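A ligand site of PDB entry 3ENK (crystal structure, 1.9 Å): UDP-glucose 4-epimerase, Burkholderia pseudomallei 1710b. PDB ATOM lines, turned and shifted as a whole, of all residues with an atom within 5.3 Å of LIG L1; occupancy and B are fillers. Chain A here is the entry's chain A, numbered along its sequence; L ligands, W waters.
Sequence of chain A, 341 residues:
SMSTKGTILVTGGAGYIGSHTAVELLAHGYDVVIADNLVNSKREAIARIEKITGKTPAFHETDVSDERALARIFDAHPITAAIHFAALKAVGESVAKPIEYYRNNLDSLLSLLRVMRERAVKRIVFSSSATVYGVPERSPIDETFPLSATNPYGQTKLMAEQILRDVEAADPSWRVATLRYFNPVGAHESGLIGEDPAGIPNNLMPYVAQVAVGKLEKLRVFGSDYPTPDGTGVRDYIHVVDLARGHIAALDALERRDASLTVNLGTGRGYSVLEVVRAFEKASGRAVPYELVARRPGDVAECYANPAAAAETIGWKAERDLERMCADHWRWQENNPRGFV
Val 91 touches LIG L1. Thr 131 touches LIG L1. ND2 of Asn 151 touches O17 of LIG L1 (3.8 Å). Tyr 153 touches LIG L1 (CE1 to O15, 3.6 Å). Asn 202 touches LIG L1. CD2 of Leu 219 touches O2 of LIG L1 (3.8 Å). Val 221 touches LIG L1 (CA to O1, 3.4 Å). Gly 233 touches LIG L1. Tyr 237 touches LIG L1 (OH to C9, 3.3 Å). Val 273 touches LIG L1. Of the 26 residues printed, 19 come within 4 Å of LIG L1.
O of Val 300 sits at hydrogen-bond distance from NH1 of Arg 235, 3.0 Å away. The side-chain carboxylate of Asp 299 lies within salt-bridge range of the guanidinium group of Arg 296 (3.3 Å). The side-chain hydroxyl of Ser 129 lies close to the backbone NH of Thr 131, at 3.0 Å. NH2 of Arg 296 lies within hydrogen-bond range of O of Asn 202 (2.6 Å). O of Gly 233 lies within hydrogen-bond range of N of Val 273 (3.0 Å). The backbone NH of Tyr 153 lies close to the side-chain amide oxygen of Asn 151 (3.3 Å).
The side-chain amide oxygen (OD1) of Asn 203 lies within hydrogen-bond range of an oxygen (O13) of LIG L1, at 2.4 Å. The guanidinium group (NE) of Arg 235 lies within salt-bridge range of an oxygen (O10) of LIG L1, 2.5 Å away. An oxygen (O3) of LIG L1 lies within hydrogen-bond range of the side-chain carboxylate (OD2) of Asp 299 (2.5 Å). A nitrogen (N2) of LIG L1 sits at hydrogen-bond distance from the backbone carbonyl oxygen (O) of Arg 220, 2.7 Å away. OG of Ser 129 sits at hydrogen-bond distance from O15 of LIG L1, at 2.8 Å. The backbone NH of Leu 204 sits at hydrogen-bond distance from an oxygen (O8) of LIG L1 (2.8 Å). The backbone NH (N) of Phe 222 lies within hydrogen-bond range of an oxygen (O1) of LIG L1, 2.9 Å away. The side-chain amide nitrogen (ND2) of Asn 183 sits at hydrogen-bond distance from an oxygen (O10) of LIG L1 (2.9 Å). The guanidinium group of Arg 296 is in salt-bridge range of an oxygen (O7) of LIG L1 (3.0 Å). OH of Tyr 153 is in hydrogen-bond range of O13 of LG2 L2.
An oxygen (O14) of LIG L1 is in hydrogen-bond range of an oxygen (O14) of LG2 L2 (2.7 Å).
Water W8 lies within hydrogen-bond range of an oxygen (O11) of LIG L1, the guanidinium group (NH2) of Arg 235 and the side-chain carboxylate (OD1) of Asp 299. Water W9 lies within hydrogen-bond range of an oxygen (O8) of LIG L1 (2.7 Å) and the side-chain amide nitrogen of Asn 183 (3.1 Å). Water W6 lies within hydrogen-bond range of the backbone carbonyl oxygen of Val 300 (2.7 Å), an oxygen (O5) of LIG L1 (2.9 Å) and the guanidinium group of Arg 235 (3.0 Å). Water W7 lies within hydrogen-bond range of the backbone carbonyl oxygen (O) of Phe 222, the backbone NH (N) of Gly 233 and an oxygen (O3) of LIG L1. Water W4 lies within hydrogen-bond range of the side-chain amide nitrogen of Asn 203 (2.6 Å) and an oxygen (O13) of LIG L1 (3.2 Å). Water W3 lies within hydrogen-bond range of the side-chain carboxylate of Asp 299 (2.7 Å), the backbone carbonyl oxygen of Phe 222 (2.7 Å), the backbone NH of Arg 296 (3.0 Å) and an oxygen (O3) of LIG L1 (3.5 Å).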
ATOM      1  N   VAL A  91     -14.643 -28.782  20.957  1.00  0.00           N
ATOM      2  CA  VAL A  91     -15.034 -28.648  22.368  1.00  0.00           C
ATOM      3  C   VAL A  91     -16.487 -29.075  22.670  1.00  0.00           C
ATOM      4  O   VAL A  91     -16.729 -29.850  23.611  1.00  0.00           O
ATOM      5  CB  VAL A  91     -14.875 -27.207  22.848  1.00  0.00           C
ATOM      6  CG1 VAL A  91     -15.530 -27.045  24.205  1.00  0.00           C
ATOM      7  CG2 VAL A  91     -13.420 -26.848  22.904  1.00  0.00           C
ATOM      8  N   SER A 129      -2.503 -26.767  23.718  1.00  0.00           N
ATOM      9  CA  SER A 129      -3.493 -25.741  23.494  1.00  0.00           C
ATOM     10  C   SER A 129      -3.548 -24.767  24.672  1.00  0.00           C
ATOM     11  O   SER A 129      -3.281 -25.167  25.807  1.00  0.00           O
ATOM     12  CB  SER A 129      -4.866 -26.386  23.325  1.00  0.00           C
ATOM     13  OG  SER A 129      -5.912 -25.432  23.337  1.00  0.00           O
ATOM     14  N   ALA A 130      -3.918 -23.508  24.413  1.00  0.00           N
ATOM     15  CA  ALA A 130      -4.189 -22.512  25.486  1.00  0.00           C
ATOM     16  C   ALA A 130      -5.350 -22.907  26.382  1.00  0.00           C
ATOM     17  O   ALA A 130      -5.584 -22.320  27.470  1.00  0.00           O
ATOM     18  CB  ALA A 130      -4.469 -21.143  24.872  1.00  0.00           C
ATOM     19  N   THR A 131      -6.125 -23.893  25.918  1.00  0.00           N
ATOM     20  CA  THR A 131      -7.178 -24.497  26.765  1.00  0.00           C
ATOM     21  C   THR A 131      -6.597 -25.047  28.072  1.00  0.00           C
ATOM     22  O   THR A 131      -7.344 -25.155  29.047  1.00  0.00           O
ATOM     23  CB  THR A 131      -7.943 -25.615  25.986  1.00  0.00           C
ATOM     24  OG1 THR A 131      -9.162 -25.912  26.653  1.00  0.00           O
ATOM     25  CG2 THR A 131      -7.111 -26.845  25.894  1.00  0.00           C
ATOM     26  N   ASN A 151     -13.303 -28.283  29.899  1.00  0.00           N
ATOM     27  CA  ASN A 151     -14.028 -29.172  28.995  1.00  0.00           C
ATOM     28  C   ASN A 151     -13.155 -30.407  28.672  1.00  0.00           C
ATOM     29  O   ASN A 151     -11.962 -30.334  28.809  1.00  0.00           O
ATOM     30  CB  ASN A 151     -14.409 -28.411  27.722  1.00  0.00           C
ATOM     31  CG  ASN A 151     -13.212 -27.907  26.962  1.00  0.00           C
ATOM     32  OD1 ASN A 151     -12.489 -28.681  26.348  1.00  0.00           O
ATOM     33  ND2 ASN A 151     -12.964 -26.597  27.017  1.00  0.00           N
ATOM     34  N   TYR A 153     -12.112 -31.965  26.020  1.00  0.00           N
ATOM     35  CA  TYR A 153     -11.053 -31.707  25.056  1.00  0.00           C
ATOM     36  C   TYR A 153      -9.823 -31.066  25.760  1.00  0.00           C
ATOM     37  O   TYR A 153      -8.696 -31.545  25.601  1.00  0.00           O
ATOM     38  CB  TYR A 153     -11.543 -30.835  23.881  1.00  0.00           C
ATOM     39  CG  TYR A 153     -10.387 -30.278  23.115  1.00  0.00           C
ATOM     40  CD1 TYR A 153     -10.008 -28.939  23.260  1.00  0.00           C
ATOM     41  CD2 TYR A 153      -9.626 -31.120  22.314  1.00  0.00           C
ATOM     42  CE1 TYR A 153      -8.906 -28.432  22.585  1.00  0.00           C
ATOM     43  CE2 TYR A 153      -8.505 -30.615  21.618  1.00  0.00           C
ATOM     44  CZ  TYR A 153      -8.167 -29.281  21.764  1.00  0.00           C
ATOM     45  OH  TYR A 153      -7.080 -28.793  21.087  1.00  0.00           O
ATOM     46  N   PHE A 182      -2.380 -20.883  20.375  1.00  0.00           N
ATOM     47  CA  PHE A 182      -3.543 -20.085  20.742  1.00  0.00           C
ATOM     48  C   PHE A 182      -4.676 -20.275  19.736  1.00  0.00           C
ATOM     49  O   PHE A 182      -5.305 -21.353  19.746  1.00  0.00           O
ATOM     50  CB  PHE A 182      -3.153 -18.643  21.126  1.00  0.00           C
ATOM     51  CG  PHE A 182      -2.645 -18.568  22.544  1.00  0.00           C
ATOM     52  CD1 PHE A 182      -1.515 -19.293  22.911  1.00  0.00           C
ATOM     53  CD2 PHE A 182      -3.368 -17.887  23.516  1.00  0.00           C
ATOM     54  CE1 PHE A 182      -1.050 -19.312  24.251  1.00  0.00           C
ATOM     55  CE2 PHE A 182      -2.892 -17.869  24.872  1.00  0.00           C
ATOM     56  CZ  PHE A 182      -1.746 -18.588  25.214  1.00  0.00           C
ATOM     57  N   ASN A 183      -4.947 -19.291  18.857  1.00  0.00           N
ATOM     58  CA  ASN A 183      -6.050 -19.448  17.914  1.00  0.00           C
ATOM     59  C   ASN A 183      -5.575 -19.353  16.458  1.00  0.00           C
ATOM     60  O   ASN A 183      -5.595 -18.264  15.857  1.00  0.00           O
ATOM     61  CB  ASN A 183      -7.176 -18.436  18.175  1.00  0.00           C
ATOM     62  CG  ASN A 183      -7.948 -18.688  19.502  1.00  0.00           C
ATOM     63  OD1 ASN A 183      -7.367 -18.689  20.590  1.00  0.00           O
ATOM     64  ND2 ASN A 183      -9.254 -18.847  19.405  1.00  0.00           N
ATOM     65  N   PRO A 201     -19.144 -24.609  10.911  1.00  0.00           N
ATOM     66  CA  PRO A 201     -17.919 -24.411  11.691  1.00  0.00           C
ATOM     67  C   PRO A 201     -18.203 -24.060  13.108  1.00  0.00           C
ATOM     68  O   PRO A 201     -19.140 -23.306  13.391  1.00  0.00           O
ATOM     69  CB  PRO A 201     -17.268 -23.197  11.010  1.00  0.00           C
ATOM     70  CG  PRO A 201     -17.856 -23.173   9.642  1.00  0.00           C
ATOM     71  CD  PRO A 201     -19.250 -23.639   9.819  1.00  0.00           C
ATOM     72  N   ASN A 202     -17.379 -24.590  14.019  1.00  0.00           N
ATOM     73  CA  ASN A 202     -17.489 -24.222  15.421  1.00  0.00           C
ATOM     74  C   ASN A 202     -16.734 -22.945  15.717  1.00  0.00           C
ATOM     75  O   ASN A 202     -17.082 -22.219  16.654  1.00  0.00           O
ATOM     76  CB  ASN A 202     -16.956 -25.334  16.325  1.00  0.00           C
ATOM     77  CG  ASN A 202     -17.674 -26.651  16.106  1.00  0.00           C
ATOM     78  OD1 ASN A 202     -17.042 -27.685  15.788  1.00  0.00           O
ATOM     79  ND2 ASN A 202     -18.986 -26.629  16.253  1.00  0.00           N
ATOM     80  N   ASN A 203     -15.690 -22.692  14.922  1.00  0.00           N
ATOM     81  CA  ASN A 203     -14.717 -21.609  15.153  1.00  0.00           C
ATOM     82  C   ASN A 203     -15.038 -20.312  14.385  1.00  0.00           C
ATOM     83  O   ASN A 203     -15.763 -20.348  13.390  1.00  0.00           O
ATOM     84  CB  ASN A 203     -13.317 -22.102  14.785  1.00  0.00           C
ATOM     85  CG  ASN A 203     -12.773 -23.113  15.784  1.00  0.00           C
ATOM     86  OD1 ASN A 203     -12.296 -22.759  16.860  1.00  0.00           O
ATOM     87  ND2 ASN A 203     -12.841 -24.397  15.418  1.00  0.00           N
ATOM     88  N   LEU A 204     -14.478 -19.206  14.840  1.00  0.00           N
ATOM     89  CA  LEU A 204     -14.787 -17.873  14.300  1.00  0.00           C
ATOM     90  C   LEU A 204     -14.384 -17.665  12.842  1.00  0.00           C
ATOM     91  O   LEU A 204     -15.254 -17.366  12.012  1.00  0.00           O
ATOM     92  CB  LEU A 204     -14.187 -16.765  15.170  1.00  0.00           C
ATOM     93  CG  LEU A 204     -14.534 -15.311  14.804  1.00  0.00           C
ATOM     94  CD1 LEU A 204     -16.054 -15.084  14.821  1.00  0.00           C
ATOM     95  CD2 LEU A 204     -13.849 -14.317  15.687  1.00  0.00           C
ATOM     96  N   MET A 205     -13.090 -17.780  12.505  1.00  0.00           N
ATOM     97  CA  MET A 205     -12.672 -17.380  11.152  1.00  0.00           C
ATOM     98  C   MET A 205     -13.320 -18.210  10.042  1.00  0.00           C
ATOM     99  O   MET A 205     -13.760 -17.622   9.044  1.00  0.00           O
ATOM    100  CB  MET A 205     -11.140 -17.246  10.987  1.00  0.00           C
ATOM    101  CG  MET A 205     -10.714 -16.485   9.678  1.00  0.00           C
ATOM    102  SD  MET A 205      -9.161 -15.533   9.686  1.00  0.00           S
ATOM    103  CE  MET A 205      -9.631 -14.214  10.827  1.00  0.00           C
ATOM    104  N   TYR A 207     -16.295 -19.559  10.109  1.00  0.00           N
ATOM    105  CA  TYR A 207     -17.680 -19.089  10.019  1.00  0.00           C
ATOM    106  C   TYR A 207     -17.762 -17.767   9.267  1.00  0.00           C
ATOM    107  O   TYR A 207     -18.575 -17.612   8.342  1.00  0.00           O
ATOM    108  CB  TYR A 207     -18.321 -18.956  11.402  1.00  0.00           C
ATOM    109  CG  TYR A 207     -19.825 -19.161  11.380  1.00  0.00           C
ATOM    110  CD1 TYR A 207     -20.681 -18.219  10.787  1.00  0.00           C
ATOM    111  CD2 TYR A 207     -20.391 -20.310  11.929  1.00  0.00           C
ATOM    112  CE1 TYR A 207     -22.058 -18.415  10.774  1.00  0.00           C
ATOM    113  CE2 TYR A 207     -21.778 -20.518  11.900  1.00  0.00           C
ATOM    114  CZ  TYR A 207     -22.592 -19.570  11.306  1.00  0.00           C
ATOM    115  OH  TYR A 207     -23.957 -19.775  11.286  1.00  0.00           O
ATOM    116  N   LEU A 219     -23.386 -14.392  10.542  1.00  0.00           N
ATOM    117  CA  LEU A 219     -22.549 -14.728  11.703  1.00  0.00           C
ATOM    118  C   LEU A 219     -23.316 -14.408  12.967  1.00  0.00           C
ATOM    119  O   LEU A 219     -23.964 -13.370  13.048  1.00  0.00           O
ATOM    120  CB  LEU A 219     -21.279 -13.915  11.651  1.00  0.00           C
ATOM    121  CG  LEU A 219     -19.986 -14.181  12.453  1.00  0.00           C
ATOM    122  CD1 LEU A 219     -19.683 -13.055  13.373  1.00  0.00           C
ATOM    123  CD2 LEU A 219     -19.826 -15.550  13.119  1.00  0.00           C
ATOM    124  N   ARG A 220     -23.242 -15.298  13.962  1.00  0.00           N
ATOM    125  CA  ARG A 220     -23.675 -15.002  15.325  1.00  0.00           C
ATOM    126  C   ARG A 220     -22.488 -14.677  16.220  1.00  0.00           C
ATOM    127  O   ARG A 220     -21.531 -15.452  16.306  1.00  0.00           O
ATOM    128  CB  ARG A 220     -24.445 -16.193  15.913  1.00  0.00           C
ATOM    129  CG  ARG A 220     -25.934 -16.227  15.604  1.00  0.00           C
ATOM    130  CD  ARG A 220     -26.216 -16.512  14.129  1.00  0.00           C
ATOM    131  NE  ARG A 220     -27.564 -17.024  13.939  1.00  0.00           N
ATOM    132  CZ  ARG A 220     -27.866 -18.313  13.783  1.00  0.00           C
ATOM    133  NH1 ARG A 220     -26.919 -19.235  13.752  1.00  0.00           N
ATOM    134  NH2 ARG A 220     -29.135 -18.671  13.619  1.00  0.00           N
ATOM    135  N   VAL A 221     -22.538 -13.516  16.868  1.00  0.00           N
ATOM    136  CA  VAL A 221     -21.504 -13.098  17.813  1.00  0.00           C
ATOM    137  C   VAL A 221     -21.938 -13.547  19.224  1.00  0.00           C
ATOM    138  O   VAL A 221     -22.996 -13.123  19.713  1.00  0.00           O
ATOM    139  CB  VAL A 221     -21.283 -11.554  17.739  1.00  0.00           C
ATOM    140  CG1 VAL A 221     -20.263 -11.091  18.762  1.00  0.00           C
ATOM    141  CG2 VAL A 221     -20.792 -11.166  16.350  1.00  0.00           C
ATOM    142  N   PHE A 222     -21.127 -14.407  19.852  1.00  0.00           N
ATOM    143  CA  PHE A 222     -21.467 -15.057  21.142  1.00  0.00           C
ATOM    144  C   PHE A 222     -21.086 -14.193  22.330  1.00  0.00           C
ATOM    145  O   PHE A 222     -19.965 -14.295  22.866  1.00  0.00           O
ATOM    146  CB  PHE A 222     -20.799 -16.452  21.286  1.00  0.00           C
ATOM    147  CG  PHE A 222     -21.124 -17.417  20.161  1.00  0.00           C
ATOM    148  CD1 PHE A 222     -22.276 -17.268  19.388  1.00  0.00           C
ATOM    149  CD2 PHE A 222     -20.271 -18.508  19.900  1.00  0.00           C
ATOM    150  CE1 PHE A 222     -22.575 -18.178  18.349  1.00  0.00           C
ATOM    151  CE2 PHE A 222     -20.573 -19.428  18.888  1.00  0.00           C
ATOM    152  CZ  PHE A 222     -21.709 -19.265  18.108  1.00  0.00           C
ATOM    153  N   GLY A 233     -15.670 -11.348  22.904  1.00  0.00           N
ATOM    154  CA  GLY A 233     -14.488 -12.099  23.341  1.00  0.00           C
ATOM    155  C   GLY A 233     -13.224 -11.668  22.641  1.00  0.00           C
ATOM    156  O   GLY A 233     -13.267 -11.247  21.479  1.00  0.00           O
ATOM    157  N   VAL A 234     -12.104 -11.755  23.349  1.00  0.00           N
ATOM    158  CA  VAL A 234     -10.823 -11.359  22.824  1.00  0.00           C
ATOM    159  C   VAL A 234      -9.919 -12.580  22.808  1.00  0.00           C
ATOM    160  O   VAL A 234      -9.819 -13.295  23.816  1.00  0.00           O
ATOM    161  CB  VAL A 234     -10.189 -10.226  23.693  1.00  0.00           C
ATOM    162  CG1 VAL A 234      -8.768  -9.916  23.259  1.00  0.00           C
ATOM    163  CG2 VAL A 234     -11.062  -8.970  23.636  1.00  0.00           C
ATOM    164  N   ARG A 235      -9.283 -12.819  21.645  1.00  0.00           N
ATOM    165  CA  ARG A 235      -8.402 -13.968  21.436  1.00  0.00           C
ATOM    166  C   ARG A 235      -7.136 -13.583  20.714  1.00  0.00           C
ATOM    167  O   ARG A 235      -7.080 -12.561  20.037  1.00  0.00           O
ATOM    168  CB  ARG A 235      -9.104 -15.073  20.607  1.00  0.00           C
ATOM    169  CG  ARG A 235     -10.351 -15.644  21.232  1.00  0.00           C
ATOM    170  CD  ARG A 235     -10.098 -16.454  22.538  1.00  0.00           C
ATOM    171  NE  ARG A 235     -11.377 -17.023  22.960  1.00  0.00           N
ATOM    172  CZ  ARG A 235     -12.207 -16.466  23.847  1.00  0.00           C
ATOM    173  NH1 ARG A 235     -11.880 -15.334  24.452  1.00  0.00           N
ATOM    174  NH2 ARG A 235     -13.355 -17.071  24.133  1.00  0.00           N
ATOM    175  N   TYR A 237      -5.237 -14.486  17.811  1.00  0.00           N
ATOM    176  CA  TYR A 237      -5.254 -15.127  16.499  1.00  0.00           C
ATOM    177  C   TYR A 237      -3.851 -15.181  15.955  1.00  0.00           C
ATOM    178  O   TYR A 237      -3.124 -14.183  15.988  1.00  0.00           O
ATOM    179  CB  TYR A 237      -6.222 -14.414  15.549  1.00  0.00           C
ATOM    180  CG  TYR A 237      -7.618 -14.481  16.063  1.00  0.00           C
ATOM    181  CD1 TYR A 237      -8.353 -15.669  15.969  1.00  0.00           C
ATOM    182  CD2 TYR A 237      -8.198 -13.384  16.742  1.00  0.00           C
ATOM    183  CE1 TYR A 237      -9.650 -15.768  16.502  1.00  0.00           C
ATOM    184  CE2 TYR A 237      -9.492 -13.467  17.256  1.00  0.00           C
ATOM    185  CZ  TYR A 237     -10.200 -14.675  17.150  1.00  0.00           C
ATOM    186  OH  TYR A 237     -11.468 -14.805  17.666  1.00  0.00           O
ATOM    187  N   VAL A 273     -13.949 -10.162  18.740  1.00  0.00           N
ATOM    188  CA  VAL A 273     -14.733 -10.726  17.627  1.00  0.00           C
ATOM    189  C   VAL A 273     -15.080  -9.655  16.580  1.00  0.00           C
ATOM    190  O   VAL A 273     -15.017  -9.897  15.372  1.00  0.00           O
ATOM    191  CB  VAL A 273     -16.044 -11.350  18.132  1.00  0.00           C
ATOM    192  CG1 VAL A 273     -16.878 -11.920  16.954  1.00  0.00           C
ATOM    193  CG2 VAL A 273     -15.763 -12.419  19.165  1.00  0.00           C
ATOM    194  N   ARG A 296     -21.657 -18.001  24.657  1.00  0.00           N
ATOM    195  CA  ARG A 296     -21.598 -19.440  24.494  1.00  0.00           C
ATOM    196  C   ARG A 296     -21.039 -20.021  25.805  1.00  0.00           C
ATOM    197  O   ARG A 296     -19.965 -19.627  26.249  1.00  0.00           O
ATOM    198  CB  ARG A 296     -20.684 -19.748  23.317  1.00  0.00           C
ATOM    199  CG  ARG A 296     -20.298 -21.196  23.100  1.00  0.00           C
ATOM    200  CD  ARG A 296     -18.854 -21.207  22.581  1.00  0.00           C
ATOM    201  NE  ARG A 296     -18.726 -21.474  21.174  1.00  0.00           N
ATOM    202  CZ  ARG A 296     -17.650 -21.234  20.420  1.00  0.00           C
ATOM    203  NH1 ARG A 296     -16.557 -20.635  20.896  1.00  0.00           N
ATOM    204  NH2 ARG A 296     -17.695 -21.593  19.144  1.00  0.00           N
ATOM    205  N   ASP A 299     -17.111 -20.122  27.303  1.00  0.00           N
ATOM    206  CA  ASP A 299     -16.204 -19.088  26.763  1.00  0.00           C
ATOM    207  C   ASP A 299     -15.604 -18.170  27.827  1.00  0.00           C
ATOM    208  O   ASP A 299     -16.320 -17.702  28.706  1.00  0.00           O
ATOM    209  CB  ASP A 299     -16.891 -18.215  25.705  1.00  0.00           C
ATOM    210  CG  ASP A 299     -16.987 -18.868  24.341  1.00  0.00           C
ATOM    211  OD1 ASP A 299     -16.547 -20.043  24.190  1.00  0.00           O
ATOM    212  OD2 ASP A 299     -17.528 -18.207  23.405  1.00  0.00           O
ATOM    213  N   VAL A 300     -14.312 -17.907  27.715  1.00  0.00           N
ATOM    214  CA  VAL A 300     -13.668 -16.835  28.503  1.00  0.00           C
ATOM    215  C   VAL A 300     -13.818 -15.476  27.809  1.00  0.00           C
ATOM    216  O   VAL A 300     -13.949 -15.411  26.588  1.00  0.00           O
ATOM    217  CB  VAL A 300     -12.171 -17.134  28.812  1.00  0.00           C
ATOM    218  CG1 VAL A 300     -12.052 -18.375  29.715  1.00  0.00           C
ATOM    219  CG2 VAL A 300     -11.338 -17.317  27.525  1.00  0.00           C
HETATM  220  N1  LIG L   1     -17.260 -16.782  18.236  1.00  0.00           N
HETATM  221  C1  LIG L   1     -18.425 -16.152  17.781  1.00  0.00           C
HETATM  222  N2  LIG L   1     -19.169 -16.740  16.872  1.00  0.00           N
HETATM  223  C2  LIG L   1     -18.801 -17.932  16.348  1.00  0.00           C
HETATM  224  C3  LIG L   1     -17.646 -18.574  16.786  1.00  0.00           C
HETATM  225  C4  LIG L   1     -16.871 -17.962  17.740  1.00  0.00           C
HETATM  226  O1  LIG L   1     -18.747 -15.052  18.253  1.00  0.00           O
HETATM  227  O2  LIG L   1     -19.519 -18.479  15.497  1.00  0.00           O
HETATM  228  C5  LIG L   1     -16.428 -16.104  19.225  1.00  0.00           C
HETATM  229  C6  LIG L   1     -16.211 -16.874  20.522  1.00  0.00           C
HETATM  230  O3  LIG L   1     -17.215 -16.550  21.499  1.00  0.00           O
HETATM  231  C7  LIG L   1     -14.800 -16.462  20.908  1.00  0.00           C
HETATM  232  C8  LIG L   1     -14.085 -16.127  19.606  1.00  0.00           C
HETATM  233  O4  LIG L   1     -15.116 -15.909  18.656  1.00  0.00           O
HETATM  234  O5  LIG L   1     -14.791 -15.274  21.724  1.00  0.00           O
HETATM  235  C9  LIG L   1     -13.219 -17.270  19.091  1.00  0.00           C
HETATM  236  O6  LIG L   1     -13.885 -18.508  19.337  1.00  0.00           O
HETATM  237  P1  LIG L   1     -13.431 -19.844  18.551  1.00  0.00           P
HETATM  238  O7  LIG L   1     -14.557 -20.842  18.710  1.00  0.00           O
HETATM  239  O8  LIG L   1     -12.869 -19.570  17.163  1.00  0.00           O
HETATM  240  O9  LIG L   1     -12.123 -20.229  19.390  1.00  0.00           O
HETATM  241  P2  LIG L   1     -12.067 -20.244  21.009  1.00  0.00           P
HETATM  242  O10 LIG L   1     -11.210 -19.141  21.585  1.00  0.00           O
HETATM  243  O11 LIG L   1     -13.404 -20.594  21.622  1.00  0.00           O
HETATM  244  O12 LIG L   1     -11.107 -21.454  21.179  1.00  0.00           O
HETATM  245  C10 LIG L   1     -11.571 -22.653  20.649  1.00  0.00           C
HETATM  246  C11 LIG L   1     -10.407 -22.957  19.721  1.00  0.00           C
HETATM  247  C12 LIG L   1      -9.229 -23.634  20.446  1.00  0.00           C
HETATM  248  C13 LIG L   1      -9.632 -24.466  21.669  1.00  0.00           C
HETATM  249  C14 LIG L   1     -10.625 -23.744  22.570  1.00  0.00           C
HETATM  250  C15 LIG L   1     -10.980 -24.554  23.817  1.00  0.00           C
HETATM  251  O13 LIG L   1     -10.961 -23.703  18.650  1.00  0.00           O
HETATM  252  O14 LIG L   1      -8.565 -24.494  19.528  1.00  0.00           O
HETATM  253  O15 LIG L   1      -8.470 -24.847  22.402  1.00  0.00           O
HETATM  254  O16 LIG L   1     -11.770 -23.544  21.750  1.00  0.00           O
HETATM  255  O17 LIG L   1     -11.868 -23.833  24.699  1.00  0.00           O
HETATM  256  P1  LG2 L   2      -7.658 -30.965  12.419  1.00  0.00           P
HETATM  257  O1  LG2 L   2      -8.867 -31.741  12.823  1.00  0.00           O
HETATM  258  O2  LG2 L   2      -7.780 -30.331  11.081  1.00  0.00           O
HETATM  259  O3  LG2 L   2      -6.365 -31.904  12.372  1.00  0.00           O
HETATM  260  C1  LG2 L   2      -6.350 -33.093  13.134  1.00  0.00           C
HETATM  261  C2  LG2 L   2      -6.142 -34.299  12.222  1.00  0.00           C
HETATM  262  O4  LG2 L   2      -6.012 -35.459  13.040  1.00  0.00           O
HETATM  263  C3  LG2 L   2      -7.338 -34.574  11.313  1.00  0.00           C
HETATM  264  O5  LG2 L   2      -6.858 -34.651   9.987  1.00  0.00           O
HETATM  265  C4  LG2 L   2      -7.881 -35.940  11.793  1.00  0.00           C
HETATM  266  O6  LG2 L   2      -8.411 -36.788  10.784  1.00  0.00           O
HETATM  267  C5  LG2 L   2      -6.664 -36.551  12.430  1.00  0.00           C
HETATM  268  N1  LG2 L   2      -6.875 -37.591  13.459  1.00  0.00           N
HETATM  269  C6  LG2 L   2      -7.675 -37.493  14.554  1.00  0.00           C
HETATM  270  N2  LG2 L   2      -7.567 -38.639  15.253  1.00  0.00           N
HETATM  271  C7  LG2 L   2      -6.702 -39.476  14.585  1.00  0.00           C
HETATM  272  C8  LG2 L   2      -6.245 -40.767  14.850  1.00  0.00           C
HETATM  273  N3  LG2 L   2      -6.659 -41.519  15.910  1.00  0.00           N
HETATM  274  N4  LG2 L   2      -5.346 -41.309  13.957  1.00  0.00           N
HETATM  275  C9  LG2 L   2      -4.903 -40.632  12.846  1.00  0.00           C
HETATM  276  N5  LG2 L   2      -5.384 -39.372  12.563  1.00  0.00           N
HETATM  277  C10 LG2 L   2      -6.263 -38.800  13.452  1.00  0.00           C
HETATM  278  O7  LG2 L   2      -7.347 -29.897  13.547  1.00  0.00           O
HETATM  279  P2  LG2 L   2      -6.174 -28.820  13.529  1.00  0.00           P
HETATM  280  O8  LG2 L   2      -6.844 -27.525  13.637  1.00  0.00           O
HETATM  281  O9  LG2 L   2      -5.110 -29.066  12.492  1.00  0.00           O
HETATM  282  O10 LG2 L   2      -5.457 -29.165  14.938  1.00  0.00           O
HETATM  283  C11 LG2 L   2      -4.291 -29.956  14.958  1.00  0.00           C
HETATM  284  C12 LG2 L   2      -3.846 -30.182  16.402  1.00  0.00           C
HETATM  285  O11 LG2 L   2      -3.708 -28.922  17.039  1.00  0.00           O
HETATM  286  C13 LG2 L   2      -4.820 -30.985  17.239  1.00  0.00           C
HETATM  287  O12 LG2 L   2      -4.049 -31.769  18.141  1.00  0.00           O
HETATM  288  C14 LG2 L   2      -5.582 -29.911  18.003  1.00  0.00           C
HETATM  289  O13 LG2 L   2      -6.113 -30.379  19.220  1.00  0.00           O
HETATM  290  C15 LG2 L   2      -4.478 -28.872  18.225  1.00  0.00           C
HETATM  291  N6  LG2 L   2      -4.911 -27.483  18.415  1.00  0.00           N
HETATM  292  C16 LG2 L   2      -5.694 -26.872  17.464  1.00  0.00           C
HETATM  293  C17 LG2 L   2      -6.064 -25.560  17.616  1.00  0.00           C
HETATM  294  C18 LG2 L   2      -6.991 -24.917  16.635  1.00  0.00           C
HETATM  295  O14 LG2 L   2      -7.696 -23.831  17.092  1.00  0.00           O
HETATM  296  N7  LG2 L   2      -7.101 -25.384  15.389  1.00  0.00           N
HETATM  297  C19 LG2 L   2      -5.636 -24.830  18.737  1.00  0.00           C
HETATM  298  C20 LG2 L   2      -4.842 -25.470  19.691  1.00  0.00           C
HETATM  299  C21 LG2 L   2      -4.444 -26.791  19.500  1.00  0.00           C
HETATM  300  O   HOH W   1     -22.064 -17.879  14.040  1.00  0.00           O
HETATM  301  O   HOH W   2     -19.859 -21.179  15.452  1.00  0.00           O
HETATM  302  O   HOH W   3     -19.162 -16.349  24.383  1.00  0.00           O
HETATM  303  O   HOH W   4     -10.616 -25.521  16.022  1.00  0.00           O
HETATM  304  O   HOH W   5      -6.052 -22.930  21.725  1.00  0.00           O
HETATM  305  O   HOH W   6     -15.644 -15.110  24.473  1.00  0.00           O
HETATM  306  O   HOH W   7     -17.447 -13.396  22.063  1.00  0.00           O
HETATM  307  O   HOH W   8     -13.760 -19.778  23.990  1.00  0.00           O
HETATM  308  O   HOH W   9     -10.236 -19.520  16.575  1.00  0.00           O
